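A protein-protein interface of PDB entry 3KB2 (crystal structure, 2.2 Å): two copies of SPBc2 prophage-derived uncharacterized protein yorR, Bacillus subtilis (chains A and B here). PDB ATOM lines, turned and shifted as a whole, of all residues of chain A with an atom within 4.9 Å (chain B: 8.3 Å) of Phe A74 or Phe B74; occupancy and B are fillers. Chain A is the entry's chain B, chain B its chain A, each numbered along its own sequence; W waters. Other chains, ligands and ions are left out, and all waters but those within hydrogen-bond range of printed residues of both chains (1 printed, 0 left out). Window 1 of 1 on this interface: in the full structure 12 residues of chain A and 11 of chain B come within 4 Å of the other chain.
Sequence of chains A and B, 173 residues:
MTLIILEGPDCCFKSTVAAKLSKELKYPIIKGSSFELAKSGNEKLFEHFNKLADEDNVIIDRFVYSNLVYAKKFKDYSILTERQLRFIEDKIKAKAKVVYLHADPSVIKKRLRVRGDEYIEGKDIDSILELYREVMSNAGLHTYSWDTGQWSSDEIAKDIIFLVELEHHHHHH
The backbone carbonyl oxygen of Ala B71 lies within hydrogen-bond range of the side-chain amino group of Lys A75 (3.2 Å).
O of Lys B73 sits at hydrogen-bond distance from N of Lys A75 (3.0 Å).
O of Ala A71 lies within hydrogen-bond range of NZ of Lys B75, 2.9 Å away.
N of Lys B75 is in hydrogen-bond range of O of Lys A73 (2.9 Å).
NZ of Lys B73 lies within salt-bridge range of OD2 of Asp B124, 3.7 Å away.
Among the printed residues, merely in contact across the chains: Phe A74 with Lys B75, Lys A73 with Phe B35, Lys A73 with Phe B74, Phe A74 with Phe B74, Lys A75 with Phe B74, Phe A74 with Lys B73, Lys A72 with Lys B75, Lys A75 with Lys B75, Phe A35 with Glu B121 and Lys A75 with Lys B72.
Of chain B, only Lys B73, Phe B74 and Lys B75 come within 4 Å of Phe A74.
Phe B74 touches just these residues of chain A: Lys A73, Phe A74 and Lys A75.
Of the printed residues of chain B, Lys A73 touches Phe B35, Phe B74 and Lys B75.
Of the printed residues of chain B, Ala A71 touches Lys B75 (2.9 Å).
Of the printed residues of chain A, Lys B72 touches Lys A75.
Printed residues of chain B within 4 Å of Lys A75: Ala B71, Lys B72, Lys B73, Phe B74 and Lys B75.
Tyr A77 touches none of the printed residues of chain B.
The nearest residue of chain B that does not touch Phe A74 is Asp B124 (6.0 Å).
The nearest printed residue of chain A that does not touch Ala B71 is Asp A76 (8.2 Å).
Hydrophobic or aromatic side chains of chain A within 4 Å of the printed part of chain B: Phe A35 and Phe A74.
Hydrophobic or aromatic side chains of chain B that line the printed part of chain A: Phe B35 and Phe B74.
Among the printed residues, 14 pairs touch across the chains.
Among the printed residues, no Asp or Glu carboxylate lies within 4 Å of a Lys or Arg side-chain nitrogen of the other chain.
Lys A72 touches Lys B75, and with the chains exchanged Lys A75 touches Lys B72.
Lys A73 touches Lys B75, and with the chains exchanged Lys A75 touches Lys B73.
Phe B74 touches its own counterpart, Phe A74.
Phe A74 touches Lys B75, and with the chains exchanged Lys A75 touches Phe B74.
Of the 14 pairs that touch across the chains among the printed residues, 12 have their exchanged pair printed and touching as well.
Water W1 bridges O of Lys B73 (2.8 Å) and O of Lys A75 (3.3 Å).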
ATOM      1  N   PHE A  35     -14.588  15.479  10.026  1.00  0.00           N
ATOM      2  CA  PHE A  35     -13.800  14.461   9.339  1.00  0.00           C
ATOM      3  C   PHE A  35     -13.343  13.369  10.300  1.00  0.00           C
ATOM      4  O   PHE A  35     -13.771  12.218  10.207  1.00  0.00           O
ATOM      5  CB  PHE A  35     -12.564  15.096   8.689  1.00  0.00           C
ATOM      6  CG  PHE A  35     -11.746  14.137   7.860  1.00  0.00           C
ATOM      7  CD1 PHE A  35     -12.143  13.796   6.574  1.00  0.00           C
ATOM      8  CD2 PHE A  35     -10.570  13.585   8.364  1.00  0.00           C
ATOM      9  CE1 PHE A  35     -11.382  12.919   5.798  1.00  0.00           C
ATOM     10  CE2 PHE A  35      -9.800  12.705   7.596  1.00  0.00           C
ATOM     11  CZ  PHE A  35     -10.208  12.374   6.311  1.00  0.00           C
ATOM     12  N   TYR A  70     -19.326  13.201   1.629  1.00  0.00           N
ATOM     13  CA  TYR A  70     -17.925  12.860   1.808  1.00  0.00           C
ATOM     14  C   TYR A  70     -17.605  11.406   2.141  1.00  0.00           C
ATOM     15  O   TYR A  70     -16.479  10.956   1.921  1.00  0.00           O
ATOM     16  CB  TYR A  70     -17.309  13.812   2.839  1.00  0.00           C
ATOM     17  CG  TYR A  70     -17.373  15.252   2.370  1.00  0.00           C
ATOM     18  CD1 TYR A  70     -16.658  15.670   1.241  1.00  0.00           C
ATOM     19  CD2 TYR A  70     -18.218  16.174   2.990  1.00  0.00           C
ATOM     20  CE1 TYR A  70     -16.794  16.967   0.733  1.00  0.00           C
ATOM     21  CE2 TYR A  70     -18.358  17.471   2.489  1.00  0.00           C
ATOM     22  CZ  TYR A  70     -17.648  17.855   1.359  1.00  0.00           C
ATOM     23  OH  TYR A  70     -17.823  19.112   0.830  1.00  0.00           O
ATOM     24  N   ALA A  71     -18.576  10.665   2.658  1.00  0.00           N
ATOM     25  CA  ALA A  71     -18.330   9.264   2.974  1.00  0.00           C
ATOM     26  C   ALA A  71     -18.059   8.510   1.675  1.00  0.00           C
ATOM     27  O   ALA A  71     -17.424   7.455   1.680  1.00  0.00           O
ATOM     28  CB  ALA A  71     -19.524   8.655   3.705  1.00  0.00           C
ATOM     29  N   LYS A  72     -18.533   9.055   0.558  1.00  0.00           N
ATOM     30  CA  LYS A  72     -18.310   8.419  -0.741  1.00  0.00           C
ATOM     31  C   LYS A  72     -16.989   8.892  -1.364  1.00  0.00           C
ATOM     32  O   LYS A  72     -16.588   8.408  -2.416  1.00  0.00           O
ATOM     33  CB  LYS A  72     -19.457   8.748  -1.712  1.00  0.00           C
ATOM     34  CG  LYS A  72     -20.855   8.325  -1.275  1.00  0.00           C
ATOM     35  CD  LYS A  72     -20.978   6.814  -1.178  1.00  0.00           C
ATOM     36  CE  LYS A  72     -22.435   6.361  -1.123  1.00  0.00           C
ATOM     37  NZ  LYS A  72     -23.159   6.862   0.082  1.00  0.00           N
ATOM     38  N   LYS A  73     -16.307   9.822  -0.708  1.00  0.00           N
ATOM     39  CA  LYS A  73     -15.055  10.363  -1.238  1.00  0.00           C
ATOM     40  C   LYS A  73     -13.816   9.849  -0.502  1.00  0.00           C
ATOM     41  O   LYS A  73     -12.807   9.505  -1.120  1.00  0.00           O
ATOM     42  CB  LYS A  73     -15.100  11.895  -1.163  1.00  0.00           C
ATOM     43  CG  LYS A  73     -13.845  12.644  -1.649  1.00  0.00           C
ATOM     44  CD  LYS A  73     -13.800  12.785  -3.178  1.00  0.00           C
ATOM     45  CE  LYS A  73     -12.548  13.535  -3.639  1.00  0.00           C
ATOM     46  NZ  LYS A  73     -12.370  14.882  -2.999  1.00  0.00           N
ATOM     47  N   PHE A  74     -13.904   9.789   0.821  1.00  0.00           N
ATOM     48  CA  PHE A  74     -12.790   9.358   1.639  1.00  0.00           C
ATOM     49  C   PHE A  74     -12.874   7.936   2.169  1.00  0.00           C
ATOM     50  O   PHE A  74     -13.946   7.452   2.526  1.00  0.00           O
ATOM     51  CB  PHE A  74     -12.644  10.304   2.822  1.00  0.00           C
ATOM     52  CG  PHE A  74     -12.521  11.741   2.437  1.00  0.00           C
ATOM     53  CD1 PHE A  74     -11.410  12.194   1.743  1.00  0.00           C
ATOM     54  CD2 PHE A  74     -13.500  12.657   2.811  1.00  0.00           C
ATOM     55  CE1 PHE A  74     -11.272  13.544   1.431  1.00  0.00           C
ATOM     56  CE2 PHE A  74     -13.369  14.004   2.504  1.00  0.00           C
ATOM     57  CZ  PHE A  74     -12.250  14.448   1.813  1.00  0.00           C
ATOM     58  N   LYS A  75     -11.722   7.278   2.235  1.00  0.00           N
ATOM     59  CA  LYS A  75     -11.655   5.925   2.761  1.00  0.00           C
ATOM     60  C   LYS A  75     -11.657   5.975   4.278  1.00  0.00           C
ATOM     61  O   LYS A  75     -11.216   6.955   4.878  1.00  0.00           O
ATOM     62  CB  LYS A  75     -10.386   5.221   2.292  1.00  0.00           C
ATOM     63  CG  LYS A  75     -10.437   4.736   0.870  1.00  0.00           C
ATOM     64  CD  LYS A  75      -9.349   3.724   0.639  1.00  0.00           C
ATOM     65  CE  LYS A  75      -9.542   3.012  -0.680  1.00  0.00           C
ATOM     66  NZ  LYS A  75      -8.518   1.951  -0.827  1.00  0.00           N
ATOM     67  N   ASP A  76     -12.135   4.898   4.888  1.00  0.00           N
ATOM     68  CA  ASP A  76     -12.203   4.805   6.341  1.00  0.00           C
ATOM     69  C   ASP A  76     -13.062   5.953   6.894  1.00  0.00           C
ATOM     70  O   ASP A  76     -12.829   6.461   7.991  1.00  0.00           O
ATOM     71  CB  ASP A  76     -10.789   4.863   6.938  1.00  0.00           C
ATOM     72  CG  ASP A  76      -9.809   3.896   6.260  1.00  0.00           C
ATOM     73  OD1 ASP A  76     -10.233   2.810   5.796  1.00  0.00           O
ATOM     74  OD2 ASP A  76      -8.600   4.220   6.208  1.00  0.00           O
ATOM     75  N   TYR A  77     -14.063   6.350   6.120  1.00  0.00           N
ATOM     76  CA  TYR A  77     -14.950   7.442   6.498  1.00  0.00           C
ATOM     77  C   TYR A  77     -16.371   6.885   6.677  1.00  0.00           C
ATOM     78  O   TYR A  77     -17.100   6.705   5.700  1.00  0.00           O
ATOM     79  CB  TYR A  77     -14.893   8.497   5.391  1.00  0.00           C
ATOM     80  CG  TYR A  77     -15.507   9.833   5.718  1.00  0.00           C
ATOM     81  CD1 TYR A  77     -16.889   9.987   5.801  1.00  0.00           C
ATOM     82  CD2 TYR A  77     -14.704  10.957   5.909  1.00  0.00           C
ATOM     83  CE1 TYR A  77     -17.457  11.227   6.063  1.00  0.00           C
ATOM     84  CE2 TYR A  77     -15.259  12.201   6.174  1.00  0.00           C
ATOM     85  CZ  TYR A  77     -16.636  12.330   6.249  1.00  0.00           C
ATOM     86  OH  TYR A  77     -17.195  13.552   6.516  1.00  0.00           O
ATOM     87  N   PHE B  35      -5.703  13.147 -10.363  1.00  0.00           N
ATOM     88  CA  PHE B  35      -6.855  12.671  -9.612  1.00  0.00           C
ATOM     89  C   PHE B  35      -7.882  12.087 -10.573  1.00  0.00           C
ATOM     90  O   PHE B  35      -8.463  11.044 -10.298  1.00  0.00           O
ATOM     91  CB  PHE B  35      -7.486  13.819  -8.820  1.00  0.00           C
ATOM     92  CG  PHE B  35      -8.478  13.374  -7.780  1.00  0.00           C
ATOM     93  CD1 PHE B  35      -8.061  13.044  -6.495  1.00  0.00           C
ATOM     94  CD2 PHE B  35      -9.837  13.317  -8.078  1.00  0.00           C
ATOM     95  CE1 PHE B  35      -8.985  12.669  -5.513  1.00  0.00           C
ATOM     96  CE2 PHE B  35     -10.772  12.942  -7.104  1.00  0.00           C
ATOM     97  CZ  PHE B  35     -10.343  12.620  -5.822  1.00  0.00           C
ATOM     98  N   ALA B  38      -6.793   8.713 -11.817  1.00  0.00           N
ATOM     99  CA  ALA B  38      -6.846   7.718 -10.759  1.00  0.00           C
ATOM    100  C   ALA B  38      -8.220   7.087 -10.634  1.00  0.00           C
ATOM    101  O   ALA B  38      -8.334   5.910 -10.312  1.00  0.00           O
ATOM    102  CB  ALA B  38      -6.435   8.340  -9.441  1.00  0.00           C
ATOM    103  N   LYS B  39      -9.261   7.869 -10.898  1.00  0.00           N
ATOM    104  CA  LYS B  39     -10.626   7.368 -10.805  1.00  0.00           C
ATOM    105  C   LYS B  39     -11.154   6.721 -12.090  1.00  0.00           C
ATOM    106  O   LYS B  39     -12.315   6.333 -12.150  1.00  0.00           O
ATOM    107  CB  LYS B  39     -11.573   8.498 -10.371  1.00  0.00           C
ATOM    108  CG  LYS B  39     -11.383   9.806 -11.133  1.00  0.00           C
ATOM    109  CD  LYS B  39     -12.690  10.619 -11.282  1.00  0.00           C
ATOM    110  CE  LYS B  39     -13.216  11.168  -9.960  1.00  0.00           C
ATOM    111  NZ  LYS B  39     -14.508  11.895 -10.147  1.00  0.00           N
ATOM    112  N   ARG B  62       5.285  14.646  -9.169  1.00  0.00           N
ATOM    113  CA  ARG B  62       4.413  13.636  -8.562  1.00  0.00           C
ATOM    114  C   ARG B  62       4.249  12.467  -9.531  1.00  0.00           C
ATOM    115  O   ARG B  62       3.901  12.661 -10.698  1.00  0.00           O
ATOM    116  CB  ARG B  62       3.055  14.231  -8.203  1.00  0.00           C
ATOM    117  CG  ARG B  62       3.163  15.339  -7.179  1.00  0.00           C
ATOM    118  CD  ARG B  62       2.006  15.290  -6.213  1.00  0.00           C
ATOM    119  NE  ARG B  62       0.744  15.500  -6.903  1.00  0.00           N
ATOM    120  CZ  ARG B  62      -0.428  15.596  -6.289  1.00  0.00           C
ATOM    121  NH1 ARG B  62      -0.496  15.501  -4.964  1.00  0.00           N
ATOM    122  NH2 ARG B  62      -1.531  15.787  -7.002  1.00  0.00           N
ATOM    123  N   SER B  66       3.339   8.873  -5.184  1.00  0.00           N
ATOM    124  CA  SER B  66       2.206   9.627  -4.667  1.00  0.00           C
ATOM    125  C   SER B  66       0.936   8.811  -4.919  1.00  0.00           C
ATOM    126  O   SER B  66      -0.013   8.891  -4.147  1.00  0.00           O
ATOM    127  CB  SER B  66       2.076  10.976  -5.369  1.00  0.00           C
ATOM    128  OG  SER B  66       3.225  11.765  -5.176  1.00  0.00           O
ATOM    129  N   ASN B  67       0.906   8.036  -6.005  1.00  0.00           N
ATOM    130  CA  ASN B  67      -0.271   7.228  -6.289  1.00  0.00           C
ATOM    131  C   ASN B  67      -0.518   6.250  -5.150  1.00  0.00           C
ATOM    132  O   ASN B  67      -1.645   6.106  -4.690  1.00  0.00           O
ATOM    133  CB  ASN B  67      -0.123   6.453  -7.590  1.00  0.00           C
ATOM    134  CG  ASN B  67      -1.270   5.497  -7.816  1.00  0.00           C
ATOM    135  OD1 ASN B  67      -2.394   5.906  -8.089  1.00  0.00           O
ATOM    136  ND2 ASN B  67      -0.993   4.216  -7.695  1.00  0.00           N
ATOM    137  N   VAL B  69       0.273   6.536  -2.088  1.00  0.00           N
ATOM    138  CA  VAL B  69      -0.145   7.280  -0.895  1.00  0.00           C
ATOM    139  C   VAL B  69      -1.633   7.634  -0.942  1.00  0.00           C
ATOM    140  O   VAL B  69      -2.413   7.235  -0.066  1.00  0.00           O
ATOM    141  CB  VAL B  69       0.689   8.604  -0.754  1.00  0.00           C
ATOM    142  CG1 VAL B  69       0.100   9.523   0.324  1.00  0.00           C
ATOM    143  CG2 VAL B  69       2.134   8.263  -0.424  1.00  0.00           C
ATOM    144  N   TYR B  70      -2.024   8.367  -1.983  1.00  0.00           N
ATOM    145  CA  TYR B  70      -3.401   8.814  -2.135  1.00  0.00           C
ATOM    146  C   TYR B  70      -4.438   7.742  -2.420  1.00  0.00           C
ATOM    147  O   TYR B  70      -5.639   7.993  -2.292  1.00  0.00           O
ATOM    148  CB  TYR B  70      -3.462   9.920  -3.192  1.00  0.00           C
ATOM    149  CG  TYR B  70      -2.729  11.171  -2.755  1.00  0.00           C
ATOM    150  CD1 TYR B  70      -3.131  11.869  -1.614  1.00  0.00           C
ATOM    151  CD2 TYR B  70      -1.607  11.633  -3.449  1.00  0.00           C
ATOM    152  CE1 TYR B  70      -2.434  12.990  -1.168  1.00  0.00           C
ATOM    153  CE2 TYR B  70      -0.903  12.760  -3.009  1.00  0.00           C
ATOM    154  CZ  TYR B  70      -1.321  13.430  -1.867  1.00  0.00           C
ATOM    155  OH  TYR B  70      -0.620  14.525  -1.410  1.00  0.00           O
ATOM    156  N   ALA B  71      -3.980   6.550  -2.795  1.00  0.00           N
ATOM    157  CA  ALA B  71      -4.892   5.451  -3.074  1.00  0.00           C
ATOM    158  C   ALA B  71      -5.422   4.904  -1.748  1.00  0.00           C
ATOM    159  O   ALA B  71      -6.468   4.257  -1.696  1.00  0.00           O
ATOM    160  CB  ALA B  71      -4.176   4.358  -3.849  1.00  0.00           C
ATOM    161  N   LYS B  72      -4.695   5.181  -0.673  1.00  0.00           N
ATOM    162  CA  LYS B  72      -5.099   4.726   0.642  1.00  0.00           C
ATOM    163  C   LYS B  72      -5.958   5.784   1.336  1.00  0.00           C
ATOM    164  O   LYS B  72      -6.394   5.589   2.473  1.00  0.00           O
ATOM    165  CB  LYS B  72      -3.865   4.423   1.495  1.00  0.00           C
ATOM    166  CG  LYS B  72      -2.903   3.420   0.884  1.00  0.00           C
ATOM    167  CD  LYS B  72      -3.546   2.058   0.706  1.00  0.00           C
ATOM    168  CE  LYS B  72      -2.578   1.078   0.060  1.00  0.00           C
ATOM    169  NZ  LYS B  72      -3.243  -0.206  -0.293  1.00  0.00           N
ATOM    170  N   LYS B  73      -6.212   6.902   0.657  1.00  0.00           N
ATOM    171  CA  LYS B  73      -7.015   7.978   1.249  1.00  0.00           C
ATOM    172  C   LYS B  73      -8.337   8.284   0.551  1.00  0.00           C
ATOM    173  O   LYS B  73      -9.290   8.732   1.187  1.00  0.00           O
ATOM    174  CB  LYS B  73      -6.194   9.269   1.328  1.00  0.00           C
ATOM    175  CG  LYS B  73      -5.669   9.605   2.716  1.00  0.00           C
ATOM    176  CD  LYS B  73      -4.733   8.531   3.243  1.00  0.00           C
ATOM    177  CE  LYS B  73      -4.270   8.835   4.670  1.00  0.00           C
ATOM    178  NZ  LYS B  73      -5.395   8.947   5.644  1.00  0.00           N
ATOM    179  N   PHE B  74      -8.396   8.042  -0.753  1.00  0.00           N
ATOM    180  CA  PHE B  74      -9.604   8.328  -1.516  1.00  0.00           C
ATOM    181  C   PHE B  74     -10.269   7.076  -2.046  1.00  0.00           C
ATOM    182  O   PHE B  74      -9.599   6.093  -2.371  1.00  0.00           O
ATOM    183  CB  PHE B  74      -9.282   9.248  -2.700  1.00  0.00           C
ATOM    184  CG  PHE B  74      -8.759  10.596  -2.297  1.00  0.00           C
ATOM    185  CD1 PHE B  74      -9.506  11.422  -1.468  1.00  0.00           C
ATOM    186  CD2 PHE B  74      -7.519  11.037  -2.741  1.00  0.00           C
ATOM    187  CE1 PHE B  74      -9.030  12.666  -1.083  1.00  0.00           C
ATOM    188  CE2 PHE B  74      -7.031  12.281  -2.362  1.00  0.00           C
ATOM    189  CZ  PHE B  74      -7.791  13.098  -1.528  1.00  0.00           C
ATOM    190  N   LYS B  75     -11.593   7.117  -2.135  1.00  0.00           N
ATOM    191  CA  LYS B  75     -12.331   5.980  -2.660  1.00  0.00           C
ATOM    192  C   LYS B  75     -12.374   6.087  -4.179  1.00  0.00           C
ATOM    193  O   LYS B  75     -12.167   7.167  -4.740  1.00  0.00           O
ATOM    194  CB  LYS B  75     -13.755   5.937  -2.090  1.00  0.00           C
ATOM    195  CG  LYS B  75     -13.836   5.618  -0.594  1.00  0.00           C
ATOM    196  CD  LYS B  75     -15.283   5.340  -0.165  1.00  0.00           C
ATOM    197  CE  LYS B  75     -15.360   4.882   1.293  1.00  0.00           C
ATOM    198  NZ  LYS B  75     -16.758   4.625   1.778  1.00  0.00           N
ATOM    199  N   ASP B  76     -12.645   4.961  -4.834  1.00  0.00           N
ATOM    200  CA  ASP B  76     -12.698   4.895  -6.289  1.00  0.00           C
ATOM    201  C   ASP B  76     -11.448   5.567  -6.858  1.00  0.00           C
ATOM    202  O   ASP B  76     -11.515   6.329  -7.827  1.00  0.00           O
ATOM    203  CB  ASP B  76     -13.959   5.589  -6.821  1.00  0.00           C
ATOM    204  CG  ASP B  76     -15.252   4.957  -6.299  1.00  0.00           C
ATOM    205  OD1 ASP B  76     -15.380   3.711  -6.328  1.00  0.00           O
ATOM    206  OD2 ASP B  76     -16.157   5.714  -5.870  1.00  0.00           O
ATOM    207  N   TYR B  77     -10.308   5.280  -6.233  1.00  0.00           N
ATOM    208  CA  TYR B  77      -9.024   5.844  -6.631  1.00  0.00           C
ATOM    209  C   TYR B  77      -8.051   4.699  -6.876  1.00  0.00           C
ATOM    210  O   TYR B  77      -7.469   4.162  -5.935  1.00  0.00           O
ATOM    211  CB  TYR B  77      -8.504   6.751  -5.513  1.00  0.00           C
ATOM    212  CG  TYR B  77      -7.274   7.548  -5.865  1.00  0.00           C
ATOM    213  CD1 TYR B  77      -6.040   6.925  -6.043  1.00  0.00           C
ATOM    214  CD2 TYR B  77      -7.340   8.935  -6.010  1.00  0.00           C
ATOM    215  CE1 TYR B  77      -4.903   7.663  -6.351  1.00  0.00           C
ATOM    216  CE2 TYR B  77      -6.210   9.679  -6.318  1.00  0.00           C
ATOM    217  CZ  TYR B  77      -4.995   9.036  -6.486  1.00  0.00           C
ATOM    218  OH  TYR B  77      -3.869   9.765  -6.783  1.00  0.00           O
ATOM    219  N   SER B  78      -7.869   4.342  -8.143  1.00  0.00           N
ATOM    220  CA  SER B  78      -6.985   3.243  -8.522  1.00  0.00           C
ATOM    221  C   SER B  78      -5.548   3.340  -8.031  1.00  0.00           C
ATOM    222  O   SER B  78      -4.967   4.421  -7.936  1.00  0.00           O
ATOM    223  CB  SER B  78      -6.961   3.086 -10.041  1.00  0.00           C
ATOM    224  OG  SER B  78      -8.253   2.782 -10.525  1.00  0.00           O
ATOM    225  N   ILE B  79      -4.976   2.179  -7.744  1.00  0.00           N
ATOM    226  CA  ILE B  79      -3.607   2.099  -7.277  1.00  0.00           C
ATOM    227  C   ILE B  79      -2.832   1.079  -8.089  1.00  0.00           C
ATOM    228  O   ILE B  79      -3.393   0.099  -8.573  1.00  0.00           O
ATOM    229  CB  ILE B  79      -3.541   1.701  -5.783  1.00  0.00           C
ATOM    230  CG1 ILE B  79      -2.090   1.694  -5.314  1.00  0.00           C
ATOM    231  CG2 ILE B  79      -4.115   0.306  -5.571  1.00  0.00           C
ATOM    232  CD1 ILE B  79      -1.975   1.694  -3.804  1.00  0.00           C
ATOM    233  N   GLU B 121      -6.291  19.990   9.037  1.00  0.00           N
ATOM    234  CA  GLU B 121      -6.491  18.610   9.465  1.00  0.00           C
ATOM    235  C   GLU B 121      -5.202  18.020  10.002  1.00  0.00           C
ATOM    236  O   GLU B 121      -4.486  17.328   9.283  1.00  0.00           O
ATOM    237  CB  GLU B 121      -6.997  17.764   8.296  1.00  0.00           C
ATOM    238  CG  GLU B 121      -8.400  18.120   7.877  1.00  0.00           C
ATOM    239  CD  GLU B 121      -9.381  17.922   9.007  1.00  0.00           C
ATOM    240  OE1 GLU B 121     -10.551  18.332   8.862  1.00  0.00           O
ATOM    241  OE2 GLU B 121      -8.978  17.348  10.044  1.00  0.00           O
ATOM    242  N   ASP B 124      -4.942  14.115   9.738  1.00  0.00           N
ATOM    243  CA  ASP B 124      -4.883  13.692   8.339  1.00  0.00           C
ATOM    244  C   ASP B 124      -3.510  13.988   7.762  1.00  0.00           C
ATOM    245  O   ASP B 124      -2.903  13.141   7.104  1.00  0.00           O
ATOM    246  CB  ASP B 124      -5.928  14.411   7.487  1.00  0.00           C
ATOM    247  CG  ASP B 124      -6.098  13.765   6.118  1.00  0.00           C
ATOM    248  OD1 ASP B 124      -6.667  14.401   5.204  1.00  0.00           O
ATOM    249  OD2 ASP B 124      -5.670  12.600   5.959  1.00  0.00           O
ATOM    250  N   ILE B 128      -0.679  11.252   6.179  1.00  0.00           N
ATOM    251  CA  ILE B 128      -0.193  11.388   4.816  1.00  0.00           C
ATOM    252  C   ILE B 128       1.325  11.477   4.805  1.00  0.00           C
ATOM    253  O   ILE B 128       1.983  10.853   3.973  1.00  0.00           O
ATOM    254  CB  ILE B 128      -0.789  12.631   4.143  1.00  0.00           C
ATOM    255  CG1 ILE B 128      -2.272  12.401   3.874  1.00  0.00           C
ATOM    256  CG2 ILE B 128      -0.071  12.918   2.830  1.00  0.00           C
ATOM    257  CD1 ILE B 128      -2.948  13.581   3.238  1.00  0.00           C
HETATM  258  O   HOH W   1      -9.320   9.494   3.863  1.00  0.00           O
